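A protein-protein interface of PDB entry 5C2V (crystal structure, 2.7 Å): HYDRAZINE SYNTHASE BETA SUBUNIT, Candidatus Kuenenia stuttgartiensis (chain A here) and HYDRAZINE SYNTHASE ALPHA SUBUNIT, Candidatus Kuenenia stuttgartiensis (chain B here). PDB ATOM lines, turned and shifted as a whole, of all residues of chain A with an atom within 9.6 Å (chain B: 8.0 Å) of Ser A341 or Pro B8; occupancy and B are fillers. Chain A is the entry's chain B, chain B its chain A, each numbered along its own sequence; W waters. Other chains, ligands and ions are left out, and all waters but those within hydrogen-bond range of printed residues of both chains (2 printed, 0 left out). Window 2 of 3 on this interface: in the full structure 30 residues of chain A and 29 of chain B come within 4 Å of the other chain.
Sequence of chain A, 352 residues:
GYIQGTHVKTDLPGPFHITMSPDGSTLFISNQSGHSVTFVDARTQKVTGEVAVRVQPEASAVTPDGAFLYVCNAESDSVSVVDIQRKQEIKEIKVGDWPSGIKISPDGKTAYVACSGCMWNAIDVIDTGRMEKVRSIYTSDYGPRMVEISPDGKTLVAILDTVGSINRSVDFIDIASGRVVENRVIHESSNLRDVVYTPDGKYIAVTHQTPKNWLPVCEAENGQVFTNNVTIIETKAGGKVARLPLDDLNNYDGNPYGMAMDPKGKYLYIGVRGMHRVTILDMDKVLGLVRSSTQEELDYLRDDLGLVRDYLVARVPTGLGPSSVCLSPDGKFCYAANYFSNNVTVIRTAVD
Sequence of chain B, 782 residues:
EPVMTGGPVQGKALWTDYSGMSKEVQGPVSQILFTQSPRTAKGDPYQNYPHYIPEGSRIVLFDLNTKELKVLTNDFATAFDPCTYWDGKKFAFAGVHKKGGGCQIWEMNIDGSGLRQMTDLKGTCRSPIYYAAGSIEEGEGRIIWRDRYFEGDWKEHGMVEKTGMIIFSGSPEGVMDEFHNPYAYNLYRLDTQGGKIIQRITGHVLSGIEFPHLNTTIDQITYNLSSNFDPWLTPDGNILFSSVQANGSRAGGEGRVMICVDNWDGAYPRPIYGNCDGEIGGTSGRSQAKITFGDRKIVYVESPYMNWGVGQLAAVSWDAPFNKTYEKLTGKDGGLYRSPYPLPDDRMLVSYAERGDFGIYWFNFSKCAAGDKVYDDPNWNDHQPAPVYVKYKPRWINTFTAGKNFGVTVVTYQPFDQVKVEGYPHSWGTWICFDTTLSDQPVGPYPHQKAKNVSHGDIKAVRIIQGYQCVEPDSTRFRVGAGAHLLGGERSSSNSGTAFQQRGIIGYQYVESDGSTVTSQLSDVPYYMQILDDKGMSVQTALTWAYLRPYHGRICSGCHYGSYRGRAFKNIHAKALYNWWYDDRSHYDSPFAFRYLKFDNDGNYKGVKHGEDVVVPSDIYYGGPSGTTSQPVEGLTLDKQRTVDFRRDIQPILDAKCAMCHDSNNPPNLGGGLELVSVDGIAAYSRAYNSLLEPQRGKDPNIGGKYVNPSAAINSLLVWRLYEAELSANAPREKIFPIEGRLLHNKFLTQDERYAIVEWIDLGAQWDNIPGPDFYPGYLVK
N of Gly A321 is in hydrogen-bond range of ND1 of His A276 (3.1 Å). The backbone carbonyl oxygen (O) of Arg A273 sits at hydrogen-bond distance from a ring nitrogen (ND1) of His A276, at 3.2 Å. N of Leu A320 is in hydrogen-bond range of OG of Ser A341, at 2.9 Å. The backbone carbonyl oxygen (O) of Leu A320 sits at hydrogen-bond distance from the backbone NH (N) of Phe A340 (3.3 Å). O of Leu A320 is in hydrogen-bond range of N of Tyr A339 (3.4 Å). The backbone carbonyl oxygen of His A276 sits at hydrogen-bond distance from the backbone NH of Thr A318 (3.3 Å).
Leu A12 touches none of the printed residues of chain B. Printed residues of chain B within 4 Å of Thr A318: Gly B6 (3.3 Å) and Gly B7 (3.8 Å). Of the printed residues of chain B, Leu A320 touches Gly B7. Ala A336 touches none of the printed residues of chain B. Ser A341 touches just one residue of chain B: Pro B8. Printed residues of chain A within 4 Å of Thr B5: His A276 (3.6 Å). Pro B8 touches one residue of chain A. No residue of chain A comes within 4 Å of Val B9. The nearest residue of chain B that does not touch Ser A341 is Gly B7 (4.7 Å). The nearest printed residue of chain A that does not touch Pro B2 is Thr A318 (6.2 Å).
Water W2 lies within hydrogen-bond range of O of Pro B8 and OG of Ser A341. Water W1 lies within hydrogen-bond range of O of Gly B7 and O of Thr A318.
Among the printed residues, pairs that only touch across the chains: Leu A320 with Gly B7, Thr A318 with Gly B6, His A276 with Thr B5, Pro A317 with Pro B2, Thr A318 with Gly B7 and Ser A341 with Pro B8.
Hydrophobic or aromatic side chains of chain B within 4 Å of the printed part of chain A: Pro B2. Among the printed residues, 7 pairs touch across the chains.
N of Gly B6 sits at hydrogen-bond distance from O of His A276, at 3.4 Å.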
ATOM      1  N   LEU A  12     -33.578  -3.401 -22.397  1.00  0.00           N
ATOM      2  CA  LEU A  12     -33.460  -2.660 -21.145  1.00  0.00           C
ATOM      3  C   LEU A  12     -32.935  -1.242 -21.355  1.00  0.00           C
ATOM      4  O   LEU A  12     -31.987  -1.034 -22.113  1.00  0.00           O
ATOM      5  CB  LEU A  12     -32.552  -3.418 -20.177  1.00  0.00           C
ATOM      6  CG  LEU A  12     -32.950  -4.876 -19.934  1.00  0.00           C
ATOM      7  CD1 LEU A  12     -31.947  -5.566 -19.029  1.00  0.00           C
ATOM      8  CD2 LEU A  12     -34.351  -4.957 -19.350  1.00  0.00           C
ATOM      9  N   PRO A  13     -33.557  -0.260 -20.681  1.00  0.00           N
ATOM     10  CA  PRO A  13     -33.204   1.161 -20.805  1.00  0.00           C
ATOM     11  C   PRO A  13     -31.801   1.501 -20.299  1.00  0.00           C
ATOM     12  O   PRO A  13     -31.109   2.288 -20.946  1.00  0.00           O
ATOM     13  CB  PRO A  13     -34.270   1.860 -19.955  1.00  0.00           C
ATOM     14  CG  PRO A  13     -34.720   0.827 -18.987  1.00  0.00           C
ATOM     15  CD  PRO A  13     -34.665  -0.470 -19.734  1.00  0.00           C
ATOM     16  N   GLY A  14     -31.388   0.925 -19.172  1.00  0.00           N
ATOM     17  CA  GLY A  14     -30.037   1.139 -18.680  1.00  0.00           C
ATOM     18  C   GLY A  14     -29.715   2.561 -18.250  1.00  0.00           C
ATOM     19  O   GLY A  14     -28.825   3.178 -18.836  1.00  0.00           O
ATOM     20  N   PRO A  15     -30.457   3.109 -17.268  1.00  0.00           N
ATOM     21  CA  PRO A  15     -30.293   4.544 -16.989  1.00  0.00           C
ATOM     22  C   PRO A  15     -28.855   4.938 -16.644  1.00  0.00           C
ATOM     23  O   PRO A  15     -28.265   4.391 -15.713  1.00  0.00           O
ATOM     24  CB  PRO A  15     -31.194   4.763 -15.768  1.00  0.00           C
ATOM     25  CG  PRO A  15     -32.113   3.582 -15.723  1.00  0.00           C
ATOM     26  CD  PRO A  15     -31.345   2.445 -16.299  1.00  0.00           C
ATOM     27  N   ARG A 273     -20.590   3.543  -7.824  1.00  0.00           N
ATOM     28  CA  ARG A 273     -21.058   2.678  -8.897  1.00  0.00           C
ATOM     29  C   ARG A 273     -20.588   1.240  -8.726  1.00  0.00           C
ATOM     30  O   ARG A 273     -21.348   0.298  -8.943  1.00  0.00           O
ATOM     31  CB  ARG A 273     -20.580   3.237 -10.240  1.00  0.00           C
ATOM     32  CG  ARG A 273     -21.341   2.747 -11.456  1.00  0.00           C
ATOM     33  CD  ARG A 273     -20.735   3.338 -12.720  1.00  0.00           C
ATOM     34  NE  ARG A 273     -21.614   3.201 -13.878  1.00  0.00           N
ATOM     35  CZ  ARG A 273     -21.584   2.174 -14.719  1.00  0.00           C
ATOM     36  NH1 ARG A 273     -20.717   1.189 -14.535  1.00  0.00           N
ATOM     37  NH2 ARG A 273     -22.421   2.133 -15.747  1.00  0.00           N
ATOM     38  N   HIS A 276     -22.203  -0.018  -5.492  1.00  0.00           N
ATOM     39  CA  HIS A 276     -23.663   0.074  -5.547  1.00  0.00           C
ATOM     40  C   HIS A 276     -24.279   0.759  -4.332  1.00  0.00           C
ATOM     41  O   HIS A 276     -25.201   0.219  -3.720  1.00  0.00           O
ATOM     42  CB  HIS A 276     -24.279  -1.321  -5.688  1.00  0.00           C
ATOM     43  CG  HIS A 276     -23.549  -2.214  -6.640  1.00  0.00           C
ATOM     44  ND1 HIS A 276     -23.383  -1.904  -7.974  1.00  0.00           N
ATOM     45  CD2 HIS A 276     -22.943  -3.408  -6.453  1.00  0.00           C
ATOM     46  CE1 HIS A 276     -22.705  -2.870  -8.565  1.00  0.00           C
ATOM     47  NE2 HIS A 276     -22.424  -3.795  -7.667  1.00  0.00           N
ATOM     48  N   PRO A 317     -27.667   1.685   0.923  1.00  0.00           N
ATOM     49  CA  PRO A 317     -27.890   0.642  -0.086  1.00  0.00           C
ATOM     50  C   PRO A 317     -28.652   1.151  -1.306  1.00  0.00           C
ATOM     51  O   PRO A 317     -29.615   1.906  -1.167  1.00  0.00           O
ATOM     52  CB  PRO A 317     -28.717  -0.401   0.670  1.00  0.00           C
ATOM     53  CG  PRO A 317     -28.320  -0.228   2.090  1.00  0.00           C
ATOM     54  CD  PRO A 317     -28.088   1.247   2.265  1.00  0.00           C
ATOM     55  N   THR A 318     -28.219   0.731  -2.490  1.00  0.00           N
ATOM     56  CA  THR A 318     -28.814   1.188  -3.740  1.00  0.00           C
ATOM     57  C   THR A 318     -28.961  -0.001  -4.688  1.00  0.00           C
ATOM     58  O   THR A 318     -28.594  -1.124  -4.341  1.00  0.00           O
ATOM     59  CB  THR A 318     -27.950   2.295  -4.392  1.00  0.00           C
ATOM     60  OG1 THR A 318     -27.378   3.117  -3.368  1.00  0.00           O
ATOM     61  CG2 THR A 318     -28.774   3.177  -5.317  1.00  0.00           C
ATOM     62  N   GLY A 319     -29.503   0.239  -5.878  1.00  0.00           N
ATOM     63  CA  GLY A 319     -29.527  -0.769  -6.919  1.00  0.00           C
ATOM     64  C   GLY A 319     -28.143  -0.905  -7.523  1.00  0.00           C
ATOM     65  O   GLY A 319     -27.196  -0.259  -7.074  1.00  0.00           O
ATOM     66  N   LEU A 320     -28.020  -1.739  -8.547  1.00  0.00           N
ATOM     67  CA  LEU A 320     -26.719  -1.993  -9.151  1.00  0.00           C
ATOM     68  C   LEU A 320     -26.328  -0.886 -10.130  1.00  0.00           C
ATOM     69  O   LEU A 320     -27.115  -0.499 -10.995  1.00  0.00           O
ATOM     70  CB  LEU A 320     -26.722  -3.355  -9.849  1.00  0.00           C
ATOM     71  CG  LEU A 320     -27.210  -4.519  -8.979  1.00  0.00           C
ATOM     72  CD1 LEU A 320     -27.053  -5.847  -9.703  1.00  0.00           C
ATOM     73  CD2 LEU A 320     -26.485  -4.545  -7.638  1.00  0.00           C
ATOM     74  N   GLY A 321     -25.104  -0.387  -9.985  1.00  0.00           N
ATOM     75  CA  GLY A 321     -24.588   0.679 -10.832  1.00  0.00           C
ATOM     76  C   GLY A 321     -25.208   2.067 -10.716  1.00  0.00           C
ATOM     77  O   GLY A 321     -25.680   2.609 -11.714  1.00  0.00           O
ATOM     78  N   PRO A 322     -25.210   2.655  -9.506  1.00  0.00           N
ATOM     79  CA  PRO A 322     -25.737   4.016  -9.342  1.00  0.00           C
ATOM     80  C   PRO A 322     -24.790   5.074  -9.909  1.00  0.00           C
ATOM     81  O   PRO A 322     -24.054   5.720  -9.164  1.00  0.00           O
ATOM     82  CB  PRO A 322     -25.872   4.158  -7.825  1.00  0.00           C
ATOM     83  CG  PRO A 322     -24.830   3.266  -7.280  1.00  0.00           C
ATOM     84  CD  PRO A 322     -24.707   2.109  -8.233  1.00  0.00           C
ATOM     85  N   SER A 323     -24.821   5.241 -11.227  1.00  0.00           N
ATOM     86  CA  SER A 323     -23.887   6.120 -11.924  1.00  0.00           C
ATOM     87  C   SER A 323     -24.167   7.611 -11.722  1.00  0.00           C
ATOM     88  O   SER A 323     -23.292   8.444 -11.962  1.00  0.00           O
ATOM     89  CB  SER A 323     -23.894   5.798 -13.421  1.00  0.00           C
ATOM     90  OG  SER A 323     -25.219   5.737 -13.920  1.00  0.00           O
ATOM     91  N   ALA A 336     -31.143   8.171  -6.978  1.00  0.00           N
ATOM     92  CA  ALA A 336     -29.972   7.536  -7.577  1.00  0.00           C
ATOM     93  C   ALA A 336     -30.355   6.628  -8.745  1.00  0.00           C
ATOM     94  O   ALA A 336     -31.166   5.715  -8.592  1.00  0.00           O
ATOM     95  CB  ALA A 336     -29.208   6.747  -6.525  1.00  0.00           C
ATOM     96  N   ALA A 337     -29.759   6.881  -9.907  1.00  0.00           N
ATOM     97  CA  ALA A 337     -30.068   6.125 -11.119  1.00  0.00           C
ATOM     98  C   ALA A 337     -29.205   4.871 -11.248  1.00  0.00           C
ATOM     99  O   ALA A 337     -27.980   4.948 -11.318  1.00  0.00           O
ATOM    100  CB  ALA A 337     -29.899   7.009 -12.346  1.00  0.00           C
ATOM    101  N   ASN A 338     -29.867   3.720 -11.297  1.00  0.00           N
ATOM    102  CA  ASN A 338     -29.212   2.418 -11.368  1.00  0.00           C
ATOM    103  C   ASN A 338     -29.366   1.763 -12.740  1.00  0.00           C
ATOM    104  O   ASN A 338     -30.480   1.390 -13.152  1.00  0.00           O
ATOM    105  CB  ASN A 338     -29.765   1.496 -10.284  1.00  0.00           C
ATOM    106  CG  ASN A 338     -29.845   2.175  -8.932  1.00  0.00           C
ATOM    107  OD1 ASN A 338     -28.965   2.952  -8.562  1.00  0.00           O
ATOM    108  ND2 ASN A 338     -30.913   1.898  -8.192  1.00  0.00           N
ATOM    109  N   TYR A 339     -28.226   1.631 -13.418  1.00  0.00           N
ATOM    110  CA  TYR A 339     -28.122   1.127 -14.787  1.00  0.00           C
ATOM    111  C   TYR A 339     -28.508  -0.341 -14.940  1.00  0.00           C
ATOM    112  O   TYR A 339     -29.377  -0.679 -15.743  1.00  0.00           O
ATOM    113  CB  TYR A 339     -26.685   1.336 -15.289  1.00  0.00           C
ATOM    114  CG  TYR A 339     -26.375   0.745 -16.651  1.00  0.00           C
ATOM    115  CD1 TYR A 339     -25.852  -0.537 -16.777  1.00  0.00           C
ATOM    116  CD2 TYR A 339     -26.580   1.482 -17.809  1.00  0.00           C
ATOM    117  CE1 TYR A 339     -25.563  -1.074 -18.019  1.00  0.00           C
ATOM    118  CE2 TYR A 339     -26.295   0.954 -19.055  1.00  0.00           C
ATOM    119  CZ  TYR A 339     -25.786  -0.324 -19.154  1.00  0.00           C
ATOM    120  OH  TYR A 339     -25.497  -0.852 -20.392  1.00  0.00           O
ATOM    121  N   PHE A 340     -27.855  -1.210 -14.175  1.00  0.00           N
ATOM    122  CA  PHE A 340     -28.061  -2.648 -14.317  1.00  0.00           C
ATOM    123  C   PHE A 340     -29.425  -3.079 -13.794  1.00  0.00           C
ATOM    124  O   PHE A 340     -30.081  -3.937 -14.383  1.00  0.00           O
ATOM    125  CB  PHE A 340     -26.955  -3.422 -13.597  1.00  0.00           C
ATOM    126  CG  PHE A 340     -25.587  -3.206 -14.180  1.00  0.00           C
ATOM    127  CD1 PHE A 340     -25.249  -3.758 -15.404  1.00  0.00           C
ATOM    128  CD2 PHE A 340     -24.639  -2.457 -13.503  1.00  0.00           C
ATOM    129  CE1 PHE A 340     -23.993  -3.561 -15.946  1.00  0.00           C
ATOM    130  CE2 PHE A 340     -23.380  -2.259 -14.038  1.00  0.00           C
ATOM    131  CZ  PHE A 340     -23.058  -2.812 -15.261  1.00  0.00           C
ATOM    132  N   SER A 341     -29.850  -2.475 -12.690  1.00  0.00           N
ATOM    133  CA  SER A 341     -31.143  -2.793 -12.098  1.00  0.00           C
ATOM    134  C   SER A 341     -32.270  -2.074 -12.832  1.00  0.00           C
ATOM    135  O   SER A 341     -33.448  -2.345 -12.592  1.00  0.00           O
ATOM    136  CB  SER A 341     -31.158  -2.426 -10.614  1.00  0.00           C
ATOM    137  OG  SER A 341     -30.198  -3.178  -9.893  1.00  0.00           O
ATOM    138  N   ASN A 342     -31.893  -1.161 -13.725  1.00  0.00           N
ATOM    139  CA  ASN A 342     -32.844  -0.388 -14.520  1.00  0.00           C
ATOM    140  C   ASN A 342     -33.869   0.346 -13.668  1.00  0.00           C
ATOM    141  O   ASN A 342     -35.066   0.292 -13.954  1.00  0.00           O
ATOM    142  CB  ASN A 342     -33.573  -1.295 -15.517  1.00  0.00           C
ATOM    143  CG  ASN A 342     -32.650  -1.867 -16.569  1.00  0.00           C
ATOM    144  OD1 ASN A 342     -31.835  -1.154 -17.151  1.00  0.00           O
ATOM    145  ND2 ASN A 342     -32.775  -3.165 -16.819  1.00  0.00           N
ATOM    146  N   ASN A 343     -33.415   1.033 -12.624  1.00  0.00           N
ATOM    147  CA  ASN A 343     -34.374   1.694 -11.737  1.00  0.00           C
ATOM    148  C   ASN A 343     -33.800   2.895 -11.000  1.00  0.00           C
ATOM    149  O   ASN A 343     -32.661   3.269 -11.221  1.00  0.00           O
ATOM    150  CB  ASN A 343     -34.941   0.687 -10.727  1.00  0.00           C
ATOM    151  CG  ASN A 343     -33.860  -0.072  -9.980  1.00  0.00           C
ATOM    152  OD1 ASN A 343     -32.713   0.366  -9.901  1.00  0.00           O
ATOM    153  ND2 ASN A 343     -34.225  -1.222  -9.426  1.00  0.00           N
ATOM    154  N   VAL A 344     -34.603   3.506 -10.135  1.00  0.00           N
ATOM    155  CA  VAL A 344     -34.149   4.662  -9.371  1.00  0.00           C
ATOM    156  C   VAL A 344     -34.424   4.476  -7.885  1.00  0.00           C
ATOM    157  O   VAL A 344     -35.552   4.187  -7.483  1.00  0.00           O
ATOM    158  CB  VAL A 344     -34.822   5.966  -9.850  1.00  0.00           C
ATOM    159  CG1 VAL A 344     -34.444   7.128  -8.940  1.00  0.00           C
ATOM    160  CG2 VAL A 344     -34.435   6.269 -11.292  1.00  0.00           C
ATOM    161  N   THR A 345     -33.385   4.638  -7.072  1.00  0.00           N
ATOM    162  CA  THR A 345     -33.525   4.532  -5.628  1.00  0.00           C
ATOM    163  C   THR A 345     -33.847   5.892  -5.017  1.00  0.00           C
ATOM    164  O   THR A 345     -33.158   6.885  -5.277  1.00  0.00           O
ATOM    165  CB  THR A 345     -32.252   3.965  -4.975  1.00  0.00           C
ATOM    166  OG1 THR A 345     -32.015   2.637  -5.461  1.00  0.00           O
ATOM    167  CG2 THR A 345     -32.397   3.923  -3.461  1.00  0.00           C
ATOM    168  N   PRO B   2     -29.118  -6.005   2.512  1.00  0.00           N
ATOM    169  CA  PRO B   2     -27.815  -5.466   2.112  1.00  0.00           C
ATOM    170  C   PRO B   2     -27.063  -4.884   3.308  1.00  0.00           C
ATOM    171  O   PRO B   2     -27.679  -4.252   4.166  1.00  0.00           O
ATOM    172  CB  PRO B   2     -28.183  -4.375   1.105  1.00  0.00           C
ATOM    173  CG  PRO B   2     -29.554  -3.945   1.506  1.00  0.00           C
ATOM    174  CD  PRO B   2     -30.237  -5.186   2.010  1.00  0.00           C
ATOM    175  N   THR B   5     -22.850  -3.618   0.749  1.00  0.00           N
ATOM    176  CA  THR B   5     -23.189  -3.079  -0.563  1.00  0.00           C
ATOM    177  C   THR B   5     -24.652  -3.339  -0.906  1.00  0.00           C
ATOM    178  O   THR B   5     -25.305  -4.173  -0.279  1.00  0.00           O
ATOM    179  CB  THR B   5     -22.303  -3.686  -1.665  1.00  0.00           C
ATOM    180  OG1 THR B   5     -22.461  -2.937  -2.874  1.00  0.00           O
ATOM    181  CG2 THR B   5     -22.690  -5.131  -1.923  1.00  0.00           C
ATOM    182  N   GLY B   6     -25.163  -2.620  -1.901  1.00  0.00           N
ATOM    183  CA  GLY B   6     -26.522  -2.825  -2.366  1.00  0.00           C
ATOM    184  C   GLY B   6     -26.678  -4.160  -3.071  1.00  0.00           C
ATOM    185  O   GLY B   6     -25.703  -4.717  -3.578  1.00  0.00           O
ATOM    186  N   GLY B   7     -27.900  -4.681  -3.098  1.00  0.00           N
ATOM    187  CA  GLY B   7     -28.165  -5.958  -3.733  1.00  0.00           C
ATOM    188  C   GLY B   7     -28.923  -5.854  -5.045  1.00  0.00           C
ATOM    189  O   GLY B   7     -29.091  -4.761  -5.586  1.00  0.00           O
ATOM    190  N   PRO B   8     -29.383  -7.002  -5.566  1.00  0.00           N
ATOM    191  CA  PRO B   8     -30.156  -7.075  -6.811  1.00  0.00           C
ATOM    192  C   PRO B   8     -31.548  -6.460  -6.680  1.00  0.00           C
ATOM    193  O   PRO B   8     -32.037  -5.834  -7.619  1.00  0.00           O
ATOM    194  CB  PRO B   8     -30.248  -8.580  -7.076  1.00  0.00           C
ATOM    195  CG  PRO B   8     -30.136  -9.204  -5.729  1.00  0.00           C
ATOM    196  CD  PRO B   8     -29.188  -8.331  -4.959  1.00  0.00           C
ATOM    197  N   VAL B   9     -32.175  -6.647  -5.522  1.00  0.00           N
ATOM    198  CA  VAL B   9     -33.497  -6.089  -5.254  1.00  0.00           C
ATOM    199  C   VAL B   9     -33.462  -5.320  -3.937  1.00  0.00           C
ATOM    200  O   VAL B   9     -32.565  -5.526  -3.119  1.00  0.00           O
ATOM    201  CB  VAL B   9     -34.586  -7.186  -5.182  1.00  0.00           C
ATOM    202  CG1 VAL B   9     -35.951  -6.610  -5.536  1.00  0.00           C
ATOM    203  CG2 VAL B   9     -34.251  -8.343  -6.108  1.00  0.00           C
ATOM    204  N   GLN B  10     -34.431  -4.435  -3.735  1.00  0.00           N
ATOM    205  CA  GLN B  10     -34.528  -3.691  -2.485  1.00  0.00           C
ATOM    206  C   GLN B  10     -34.812  -4.644  -1.328  1.00  0.00           C
ATOM    207  O   GLN B  10     -35.779  -5.406  -1.362  1.00  0.00           O
ATOM    208  CB  GLN B  10     -35.616  -2.619  -2.578  1.00  0.00           C
ATOM    209  CG  GLN B  10     -35.833  -1.832  -1.296  1.00  0.00           C
ATOM    210  CD  GLN B  10     -36.918  -0.780  -1.439  1.00  0.00           C
ATOM    211  OE1 GLN B  10     -37.364  -0.478  -2.546  1.00  0.00           O
ATOM    212  NE2 GLN B  10     -37.349  -0.216  -0.315  1.00  0.00           N
ATOM    213  N   GLY B  11     -33.965  -4.595  -0.304  1.00  0.00           N
ATOM    214  CA  GLY B  11     -34.104  -5.479   0.840  1.00  0.00           C
ATOM    215  C   GLY B  11     -33.371  -6.797   0.668  1.00  0.00           C
ATOM    216  O   GLY B  11     -33.388  -7.645   1.560  1.00  0.00           O
ATOM    217  N   LYS B  12     -32.726  -6.972  -0.481  1.00  0.00           N
ATOM    218  CA  LYS B  12     -31.976  -8.192  -0.762  1.00  0.00           C
ATOM    219  C   LYS B  12     -30.492  -7.894  -0.944  1.00  0.00           C
ATOM    220  O   LYS B  12     -30.110  -6.769  -1.270  1.00  0.00           O
ATOM    221  CB  LYS B  12     -32.531  -8.894  -2.003  1.00  0.00           C
ATOM    222  CG  LYS B  12     -33.795  -9.698  -1.744  1.00  0.00           C
ATOM    223  CD  LYS B  12     -33.526 -10.843  -0.779  1.00  0.00           C
ATOM    224  CE  LYS B  12     -34.776 -11.678  -0.543  1.00  0.00           C
ATOM    225  NZ  LYS B  12     -34.515 -12.824   0.374  1.00  0.00           N
ATOM    226  N   ALA B  13     -29.659  -8.907  -0.731  1.00  0.00           N
ATOM    227  CA  ALA B  13     -28.212  -8.724  -0.751  1.00  0.00           C
ATOM    228  C   ALA B  13     -27.546  -9.415  -1.938  1.00  0.00           C
ATOM    229  O   ALA B  13     -28.034 -10.428  -2.440  1.00  0.00           O
ATOM    230  CB  ALA B  13     -27.604  -9.225   0.549  1.00  0.00           C
ATOM    231  N   LEU B  14     -26.428  -8.848  -2.379  1.00  0.00           N
ATOM    232  CA  LEU B  14     -25.614  -9.446  -3.427  1.00  0.00           C
ATOM    233  C   LEU B  14     -24.815 -10.607  -2.847  1.00  0.00           C
ATOM    234  O   LEU B  14     -24.492 -10.605  -1.661  1.00  0.00           O
ATOM    235  CB  LEU B  14     -24.678  -8.400  -4.037  1.00  0.00           C
ATOM    236  CG  LEU B  14     -24.389  -8.481  -5.535  1.00  0.00           C
ATOM    237  CD1 LEU B  14     -25.677  -8.366  -6.333  1.00  0.00           C
ATOM    238  CD2 LEU B  14     -23.404  -7.392  -5.941  1.00  0.00           C
ATOM    239  N   TRP B  15     -24.491 -11.597  -3.676  1.00  0.00           N
ATOM    240  CA  TRP B  15     -23.743 -12.761  -3.204  1.00  0.00           C
ATOM    241  C   TRP B  15     -22.318 -12.384  -2.809  1.00  0.00           C
ATOM    242  O   TRP B  15     -21.628 -13.149  -2.134  1.00  0.00           O
ATOM    243  CB  TRP B  15     -23.720 -13.864  -4.266  1.00  0.00           C
ATOM    244  CG  TRP B  15     -23.231 -13.427  -5.617  1.00  0.00           C
ATOM    245  CD1 TRP B  15     -23.995 -13.003  -6.665  1.00  0.00           C
ATOM    246  CD2 TRP B  15     -21.870 -13.384  -6.071  1.00  0.00           C
ATOM    247  NE1 TRP B  15     -23.196 -12.694  -7.739  1.00  0.00           N
ATOM    248  CE2 TRP B  15     -21.889 -12.918  -7.400  1.00  0.00           C
ATOM    249  CE3 TRP B  15     -20.641 -13.688  -5.479  1.00  0.00           C
ATOM    250  CZ2 TRP B  15     -20.725 -12.753  -8.150  1.00  0.00           C
ATOM    251  CZ3 TRP B  15     -19.486 -13.524  -6.226  1.00  0.00           C
ATOM    252  CH2 TRP B  15     -19.537 -13.059  -7.546  1.00  0.00           C
ATOM    253  N   MET B  21     -25.527 -11.830   2.999  1.00  0.00           N
ATOM    254  CA  MET B  21     -25.859 -13.203   2.638  1.00  0.00           C
ATOM    255  C   MET B  21     -25.895 -14.082   3.881  1.00  0.00           C
ATOM    256  O   MET B  21     -26.675 -15.028   3.953  1.00  0.00           O
ATOM    257  CB  MET B  21     -24.860 -13.765   1.623  1.00  0.00           C
ATOM    258  CG  MET B  21     -24.894 -13.080   0.265  1.00  0.00           C
ATOM    259  SD  MET B  21     -26.504 -13.115  -0.543  1.00  0.00           S
ATOM    260  CE  MET B  21     -26.708 -14.874  -0.809  1.00  0.00           C
ATOM    261  N   GLU B  24     -29.247 -13.523   5.309  1.00  0.00           N
ATOM    262  CA  GLU B  24     -30.319 -14.159   4.550  1.00  0.00           C
ATOM    263  C   GLU B  24     -30.303 -15.686   4.649  1.00  0.00           C
ATOM    264  O   GLU B  24     -31.346 -16.330   4.529  1.00  0.00           O
ATOM    265  CB  GLU B  24     -30.247 -13.738   3.080  1.00  0.00           C
ATOM    266  CG  GLU B  24     -30.516 -12.258   2.847  1.00  0.00           C
ATOM    267  CD  GLU B  24     -30.466 -11.878   1.378  1.00  0.00           C
ATOM    268  OE1 GLU B  24     -30.253 -12.776   0.537  1.00  0.00           O
ATOM    269  OE2 GLU B  24     -30.641 -10.681   1.067  1.00  0.00           O
HETATM  270  O   HOH W   1     -30.730  -2.818  -4.635  1.00  0.00           O
HETATM  271  O   HOH W   2     -31.031  -5.727  -9.845  1.00  0.00           O
